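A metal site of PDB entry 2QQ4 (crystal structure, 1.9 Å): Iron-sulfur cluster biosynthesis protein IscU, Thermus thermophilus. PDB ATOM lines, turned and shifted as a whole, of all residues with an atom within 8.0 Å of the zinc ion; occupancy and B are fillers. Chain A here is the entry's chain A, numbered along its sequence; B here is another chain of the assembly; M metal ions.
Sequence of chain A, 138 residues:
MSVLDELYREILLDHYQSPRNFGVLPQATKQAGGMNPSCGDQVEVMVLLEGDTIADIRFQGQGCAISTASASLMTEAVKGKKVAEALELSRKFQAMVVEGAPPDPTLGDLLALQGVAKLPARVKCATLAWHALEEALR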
ATOM      1  N   ASN A  36     -22.444  20.662 -32.372  1.00  0.00           N
ATOM      2  CA  ASN A  36     -22.475  22.018 -32.927  1.00  0.00           C
ATOM      3  C   ASN A  36     -21.136  21.995 -33.668  1.00  0.00           C
ATOM      4  O   ASN A  36     -20.098  22.311 -33.084  1.00  0.00           O
ATOM      5  CB  ASN A  36     -22.456  23.070 -31.820  1.00  0.00           C
ATOM      6  CG  ASN A  36     -23.839  23.400 -31.277  1.00  0.00           C
ATOM      7  OD1 ASN A  36     -23.975  24.029 -30.229  1.00  0.00           O
ATOM      8  ND2 ASN A  36     -24.867  22.994 -32.009  1.00  0.00           N
ATOM      9  N   SER A  38     -19.410  23.903 -35.444  1.00  0.00           N
ATOM     10  CA  SER A  38     -18.498  25.042 -35.304  1.00  0.00           C
ATOM     11  C   SER A  38     -18.068  25.339 -33.868  1.00  0.00           C
ATOM     12  O   SER A  38     -16.871  25.265 -33.560  1.00  0.00           O
ATOM     13  CB  SER A  38     -19.145  26.286 -35.924  1.00  0.00           C
ATOM     14  OG  SER A  38     -20.420  26.559 -35.372  1.00  0.00           O
ATOM     15  N   CYS A  39     -19.009  25.684 -33.002  1.00  0.00           N
ATOM     16  CA  CYS A  39     -18.678  26.003 -31.616  1.00  0.00           C
ATOM     17  C   CYS A  39     -17.859  24.887 -30.975  1.00  0.00           C
ATOM     18  O   CYS A  39     -17.131  25.121 -30.010  1.00  0.00           O
ATOM     19  CB  CYS A  39     -19.950  26.249 -30.780  1.00  0.00           C
ATOM     20  SG  CYS A  39     -19.661  26.893 -29.089  1.00  0.00           S
ATOM     21  N   GLY A  40     -17.970  23.692 -31.523  1.00  0.00           N
ATOM     22  CA  GLY A  40     -17.231  22.565 -30.991  1.00  0.00           C
ATOM     23  C   GLY A  40     -17.933  21.880 -29.827  1.00  0.00           C
ATOM     24  O   GLY A  40     -17.364  20.982 -29.198  1.00  0.00           O
ATOM     25  N   ASP A  41     -19.156  22.298 -29.533  1.00  0.00           N
ATOM     26  CA  ASP A  41     -19.885  21.675 -28.446  1.00  0.00           C
ATOM     27  C   ASP A  41     -20.375  20.309 -28.911  1.00  0.00           C
ATOM     28  O   ASP A  41     -20.827  20.151 -30.051  1.00  0.00           O
ATOM     29  CB  ASP A  41     -21.103  22.495 -28.012  1.00  0.00           C
ATOM     30  CG  ASP A  41     -20.770  23.947 -27.686  1.00  0.00           C
ATOM     31  OD1 ASP A  41     -19.675  24.215 -27.144  1.00  0.00           O
ATOM     32  OD2 ASP A  41     -21.628  24.809 -27.962  1.00  0.00           O
ATOM     33  N   GLN A  42     -20.285  19.338 -28.021  1.00  0.00           N
ATOM     34  CA  GLN A  42     -20.743  17.991 -28.323  1.00  0.00           C
ATOM     35  C   GLN A  42     -21.429  17.461 -27.074  1.00  0.00           C
ATOM     36  O   GLN A  42     -20.990  17.724 -25.947  1.00  0.00           O
ATOM     37  CB  GLN A  42     -19.579  17.090 -28.719  1.00  0.00           C
ATOM     38  CG  GLN A  42     -18.526  16.917 -27.646  1.00  0.00           C
ATOM     39  CD  GLN A  42     -17.448  15.937 -28.057  1.00  0.00           C
ATOM     40  OE1 GLN A  42     -16.516  15.671 -27.293  1.00  0.00           O
ATOM     41  NE2 GLN A  42     -17.554  15.394 -29.267  1.00  0.00           N
ATOM     42  N   GLN A  62     -18.443  17.961 -23.955  1.00  0.00           N
ATOM     43  CA  GLN A  62     -17.548  19.053 -23.632  1.00  0.00           C
ATOM     44  C   GLN A  62     -18.074  20.203 -24.470  1.00  0.00           C
ATOM     45  O   GLN A  62     -18.714  19.993 -25.497  1.00  0.00           O
ATOM     46  CB  GLN A  62     -16.131  18.719 -24.082  1.00  0.00           C
ATOM     47  CG  GLN A  62     -15.654  17.319 -23.760  1.00  0.00           C
ATOM     48  CD  GLN A  62     -14.943  17.227 -22.429  1.00  0.00           C
ATOM     49  OE1 GLN A  62     -15.532  17.467 -21.370  1.00  0.00           O
ATOM     50  NE2 GLN A  62     -13.659  16.881 -22.472  1.00  0.00           N
ATOM     51  N   GLY A  63     -17.773  21.423 -24.053  1.00  0.00           N
ATOM     52  CA  GLY A  63     -18.234  22.572 -24.806  1.00  0.00           C
ATOM     53  C   GLY A  63     -18.224  23.807 -23.950  1.00  0.00           C
ATOM     54  O   GLY A  63     -17.626  23.829 -22.862  1.00  0.00           O
ATOM     55  N   CYS A  64     -18.884  24.844 -24.441  1.00  0.00           N
ATOM     56  CA  CYS A  64     -18.953  26.118 -23.754  1.00  0.00           C
ATOM     57  C   CYS A  64     -19.828  26.022 -22.508  1.00  0.00           C
ATOM     58  O   CYS A  64     -20.628  25.092 -22.358  1.00  0.00           O
ATOM     59  CB  CYS A  64     -19.531  27.172 -24.693  1.00  0.00           C
ATOM     60  SG  CYS A  64     -21.287  26.931 -25.026  1.00  0.00           S
ATOM     61  N   ALA A  65     -19.663  26.994 -21.614  1.00  0.00           N
ATOM     62  CA  ALA A  65     -20.413  27.047 -20.374  1.00  0.00           C
ATOM     63  C   ALA A  65     -21.933  26.964 -20.593  1.00  0.00           C
ATOM     64  O   ALA A  65     -22.635  26.300 -19.847  1.00  0.00           O
ATOM     65  CB  ALA A  65     -20.068  28.342 -19.624  1.00  0.00           C
ATOM     66  N   ILE A  66     -22.436  27.667 -21.593  1.00  0.00           N
ATOM     67  CA  ILE A  66     -23.869  27.639 -21.866  1.00  0.00           C
ATOM     68  C   ILE A  66     -24.355  26.233 -22.196  1.00  0.00           C
ATOM     69  O   ILE A  66     -25.376  25.792 -21.672  1.00  0.00           O
ATOM     70  CB  ILE A  66     -24.251  28.574 -23.047  1.00  0.00           C
ATOM     71  CG1 ILE A  66     -23.985  30.041 -22.667  1.00  0.00           C
ATOM     72  CG2 ILE A  66     -25.718  28.366 -23.411  1.00  0.00           C
ATOM     73  CD1 ILE A  66     -24.089  31.000 -23.842  1.00  0.00           C
ATOM     74  N   SER A  67     -23.637  25.507 -23.049  1.00  0.00           N
ATOM     75  CA  SER A  67     -24.085  24.165 -23.413  1.00  0.00           C
ATOM     76  C   SER A  67     -24.063  23.207 -22.231  1.00  0.00           C
ATOM     77  O   SER A  67     -24.956  22.389 -22.075  1.00  0.00           O
ATOM     78  CB  SER A  67     -23.242  23.587 -24.574  1.00  0.00           C
ATOM     79  OG  SER A  67     -21.867  23.515 -24.269  1.00  0.00           O
ATOM     80  N   THR A  68     -23.058  23.334 -21.368  1.00  0.00           N
ATOM     81  CA  THR A  68     -22.963  22.456 -20.203  1.00  0.00           C
ATOM     82  C   THR A  68     -24.111  22.714 -19.235  1.00  0.00           C
ATOM     83  O   THR A  68     -24.805  21.793 -18.808  1.00  0.00           O
ATOM     84  CB  THR A  68     -21.610  22.651 -19.484  1.00  0.00           C
ATOM     85  OG1 THR A  68     -20.543  22.356 -20.393  1.00  0.00           O
ATOM     86  CG2 THR A  68     -21.506  21.727 -18.280  1.00  0.00           C
ATOM     87  N   ALA A 121     -27.014  33.803 -32.364  1.00  0.00           N
ATOM     88  CA  ALA A 121     -25.908  32.909 -32.688  1.00  0.00           C
ATOM     89  C   ALA A 121     -25.536  31.915 -31.595  1.00  0.00           C
ATOM     90  O   ALA A 121     -24.912  30.893 -31.880  1.00  0.00           O
ATOM     91  CB  ALA A 121     -24.689  33.733 -33.089  1.00  0.00           C
ATOM     92  N   ARG A 122     -25.910  32.188 -30.343  1.00  0.00           N
ATOM     93  CA  ARG A 122     -25.588  31.275 -29.252  1.00  0.00           C
ATOM     94  C   ARG A 122     -26.769  30.367 -28.862  1.00  0.00           C
ATOM     95  O   ARG A 122     -26.652  29.492 -27.996  1.00  0.00           O
ATOM     96  CB  ARG A 122     -25.136  32.079 -28.029  1.00  0.00           C
ATOM     97  CG  ARG A 122     -23.905  32.965 -28.278  1.00  0.00           C
ATOM     98  CD  ARG A 122     -23.743  33.968 -27.147  1.00  0.00           C
ATOM     99  NE  ARG A 122     -22.713  34.986 -27.388  1.00  0.00           N
ATOM    100  CZ  ARG A 122     -22.731  35.858 -28.386  1.00  0.00           C
ATOM    101  NH1 ARG A 122     -23.730  35.863 -29.264  1.00  0.00           N
ATOM    102  NH2 ARG A 122     -21.753  36.750 -28.508  1.00  0.00           N
ATOM    103  N   VAL A 123     -27.910  30.571 -29.495  1.00  0.00           N
ATOM    104  CA  VAL A 123     -29.074  29.769 -29.189  1.00  0.00           C
ATOM    105  C   VAL A 123     -28.790  28.269 -29.380  1.00  0.00           C
ATOM    106  O   VAL A 123     -29.300  27.439 -28.630  1.00  0.00           O
ATOM    107  CB  VAL A 123     -30.301  30.212 -30.041  1.00  0.00           C
ATOM    108  CG1 VAL A 123     -31.430  29.163 -29.968  1.00  0.00           C
ATOM    109  CG2 VAL A 123     -30.824  31.561 -29.528  1.00  0.00           C
ATOM    110  N   LYS A 124     -27.967  27.927 -30.363  1.00  0.00           N
ATOM    111  CA  LYS A 124     -27.640  26.517 -30.610  1.00  0.00           C
ATOM    112  C   LYS A 124     -26.893  25.879 -29.447  1.00  0.00           C
ATOM    113  O   LYS A 124     -26.949  24.672 -29.249  1.00  0.00           O
ATOM    114  CB  LYS A 124     -26.806  26.363 -31.884  1.00  0.00           C
ATOM    115  CG  LYS A 124     -25.524  27.175 -31.892  1.00  0.00           C
ATOM    116  CD  LYS A 124     -24.753  26.984 -33.199  1.00  0.00           C
ATOM    117  CE  LYS A 124     -24.302  28.320 -33.802  1.00  0.00           C
ATOM    118  NZ  LYS A 124     -25.426  29.163 -34.385  1.00  0.00           N
ATOM    119  N   CYS A 125     -26.172  26.701 -28.676  1.00  0.00           N
ATOM    120  CA  CYS A 125     -25.438  26.170 -27.536  1.00  0.00           C
ATOM    121  C   CYS A 125     -26.432  25.716 -26.465  1.00  0.00           C
ATOM    122  O   CYS A 125     -26.179  24.752 -25.732  1.00  0.00           O
ATOM    123  CB  CYS A 125     -24.499  27.234 -26.970  1.00  0.00           C
ATOM    124  SG  CYS A 125     -23.304  27.830 -28.180  1.00  0.00           S
ATOM    125  N   ALA A 126     -27.576  26.402 -26.396  1.00  0.00           N
ATOM    126  CA  ALA A 126     -28.602  26.065 -25.399  1.00  0.00           C
ATOM    127  C   ALA A 126     -29.500  24.903 -25.814  1.00  0.00           C
ATOM    128  O   ALA A 126     -29.907  24.098 -24.991  1.00  0.00           O
ATOM    129  CB  ALA A 126     -29.459  27.292 -25.098  1.00  0.00           C
ATOM    130  N   LEU A 128     -28.716  22.403 -28.061  1.00  0.00           N
ATOM    131  CA  LEU A 128     -28.010  21.161 -28.382  1.00  0.00           C
ATOM    132  C   LEU A 128     -28.445  19.960 -27.544  1.00  0.00           C
ATOM    133  O   LEU A 128     -28.834  18.920 -28.082  1.00  0.00           O
ATOM    134  CB  LEU A 128     -26.493  21.356 -28.247  1.00  0.00           C
ATOM    135  CG  LEU A 128     -25.623  20.152 -28.645  1.00  0.00           C
ATOM    136  CD1 LEU A 128     -25.940  19.775 -30.067  1.00  0.00           C
ATOM    137  CD2 LEU A 128     -24.148  20.490 -28.514  1.00  0.00           C
ATOM    138  N   TYR B   8     -20.579  35.280 -17.722  1.00  0.00           N
ATOM    139  CA  TYR B   8     -19.288  35.514 -18.364  1.00  0.00           C
ATOM    140  C   TYR B   8     -18.292  36.146 -17.404  1.00  0.00           C
ATOM    141  O   TYR B   8     -17.132  35.753 -17.341  1.00  0.00           O
ATOM    142  CB  TYR B   8     -19.449  36.427 -19.583  1.00  0.00           C
ATOM    143  CG  TYR B   8     -20.005  35.733 -20.822  1.00  0.00           C
ATOM    144  CD1 TYR B   8     -20.753  36.447 -21.757  1.00  0.00           C
ATOM    145  CD2 TYR B   8     -19.775  34.378 -21.047  1.00  0.00           C
ATOM    146  CE1 TYR B   8     -21.272  35.834 -22.899  1.00  0.00           C
ATOM    147  CE2 TYR B   8     -20.288  33.753 -22.192  1.00  0.00           C
ATOM    148  CZ  TYR B   8     -21.030  34.483 -23.112  1.00  0.00           C
ATOM    149  OH  TYR B   8     -21.538  33.873 -24.243  1.00  0.00           O
ATOM    150  N   PRO B 105     -20.275  32.023 -32.237  1.00  0.00           N
ATOM    151  CA  PRO B 105     -20.292  31.219 -31.026  1.00  0.00           C
ATOM    152  C   PRO B 105     -19.121  30.239 -30.925  1.00  0.00           C
ATOM    153  O   PRO B 105     -18.891  29.663 -29.859  1.00  0.00           O
ATOM    154  CB  PRO B 105     -21.633  30.504 -31.109  1.00  0.00           C
ATOM    155  CG  PRO B 105     -21.788  30.299 -32.581  1.00  0.00           C
ATOM    156  CD  PRO B 105     -21.382  31.653 -33.129  1.00  0.00           C
ATOM    157  N   THR B 106     -18.387  30.074 -32.019  1.00  0.00           N
ATOM    158  CA  THR B 106     -17.257  29.151 -32.039  1.00  0.00           C
ATOM    159  C   THR B 106     -16.116  29.643 -31.154  1.00  0.00           C
ATOM    160  O   THR B 106     -15.062  29.023 -31.094  1.00  0.00           O
ATOM    161  CB  THR B 106     -16.711  28.954 -33.471  1.00  0.00           C
ATOM    162  OG1 THR B 106     -15.713  29.939 -33.754  1.00  0.00           O
ATOM    163  CG2 THR B 106     -17.828  29.076 -34.489  1.00  0.00           C
ATOM    164  N   LEU B 107     -16.341  30.772 -30.482  1.00  0.00           N
ATOM    165  CA  LEU B 107     -15.348  31.324 -29.576  1.00  0.00           C
ATOM    166  C   LEU B 107     -15.676  30.828 -28.179  1.00  0.00           C
ATOM    167  O   LEU B 107     -14.847  30.879 -27.281  1.00  0.00           O
ATOM    168  CB  LEU B 107     -15.362  32.852 -29.616  1.00  0.00           C
ATOM    169  CG  LEU B 107     -14.598  33.495 -30.769  1.00  0.00           C
ATOM    170  CD1 LEU B 107     -14.772  35.000 -30.750  1.00  0.00           C
ATOM    171  CD2 LEU B 107     -13.118  33.123 -30.656  1.00  0.00           C
ATOM    172  N   GLY B 108     -16.916  30.362 -28.023  1.00  0.00           N
ATOM    173  CA  GLY B 108     -17.373  29.830 -26.745  1.00  0.00           C
ATOM    174  C   GLY B 108     -17.135  30.727 -25.547  1.00  0.00           C
ATOM    175  O   GLY B 108     -17.541  31.893 -25.536  1.00  0.00           O
ATOM    176  N   ASP B 109     -16.485  30.171 -24.532  1.00  0.00           N
ATOM    177  CA  ASP B 109     -16.215  30.924 -23.320  1.00  0.00           C
ATOM    178  C   ASP B 109     -15.362  32.160 -23.571  1.00  0.00           C
ATOM    179  O   ASP B 109     -15.378  33.095 -22.777  1.00  0.00           O
ATOM    180  CB  ASP B 109     -15.558  30.025 -22.283  1.00  0.00           C
ATOM    181  CG  ASP B 109     -16.506  28.961 -21.740  1.00  0.00           C
ATOM    182  OD1 ASP B 109     -17.723  29.073 -22.007  1.00  0.00           O
ATOM    183  OD2 ASP B 109     -16.035  28.039 -21.039  1.00  0.00           O
ATOM    184  N   LEU B 111     -15.952  34.362 -25.494  1.00  0.00           N
ATOM    185  CA  LEU B 111     -16.847  35.482 -25.691  1.00  0.00           C
ATOM    186  C   LEU B 111     -16.900  36.375 -24.444  1.00  0.00           C
ATOM    187  O   LEU B 111     -17.302  37.528 -24.508  1.00  0.00           O
ATOM    188  CB  LEU B 111     -18.252  34.981 -26.040  1.00  0.00           C
ATOM    189  CG  LEU B 111     -18.369  34.315 -27.418  1.00  0.00           C
ATOM    190  CD1 LEU B 111     -19.802  33.883 -27.677  1.00  0.00           C
ATOM    191  CD2 LEU B 111     -17.911  35.296 -28.492  1.00  0.00           C
HETATM  192 ZN    ZN M   1     -21.472  26.631 -27.387  1.00  0.00          ZN
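SG of Cys 64 sits close to N of Ile 66, at 3.7 Å. The backbone carbonyl oxygen (O) of Asp 41 sits at hydrogen-bond distance from the backbone NH (N) of Asn 36 (2.9 Å). The side-chain hydroxyl of Thr 68 sits at hydrogen-bond distance from the backbone carbonyl oxygen of Cys 64 (3.4 Å). The backbone carbonyl oxygen (O) of Arg 122 lies close to the side-chain sulfur (SG) of Cys 125 (3.7 Å). O of Cys 64 lies within hydrogen-bond range of OG of Ser 67. SG of Cys 39 lies close to O of Pro 105 of chain B.
The zinc ion is bound by OD2 of Asp 41 (1.9 Å), SG of Cys 125 (2.3 Å), SG of Cys 64 (2.4 Å) and SG of Cys 39 (2.5 Å). The zinc ion has four donor atoms within binding distance.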
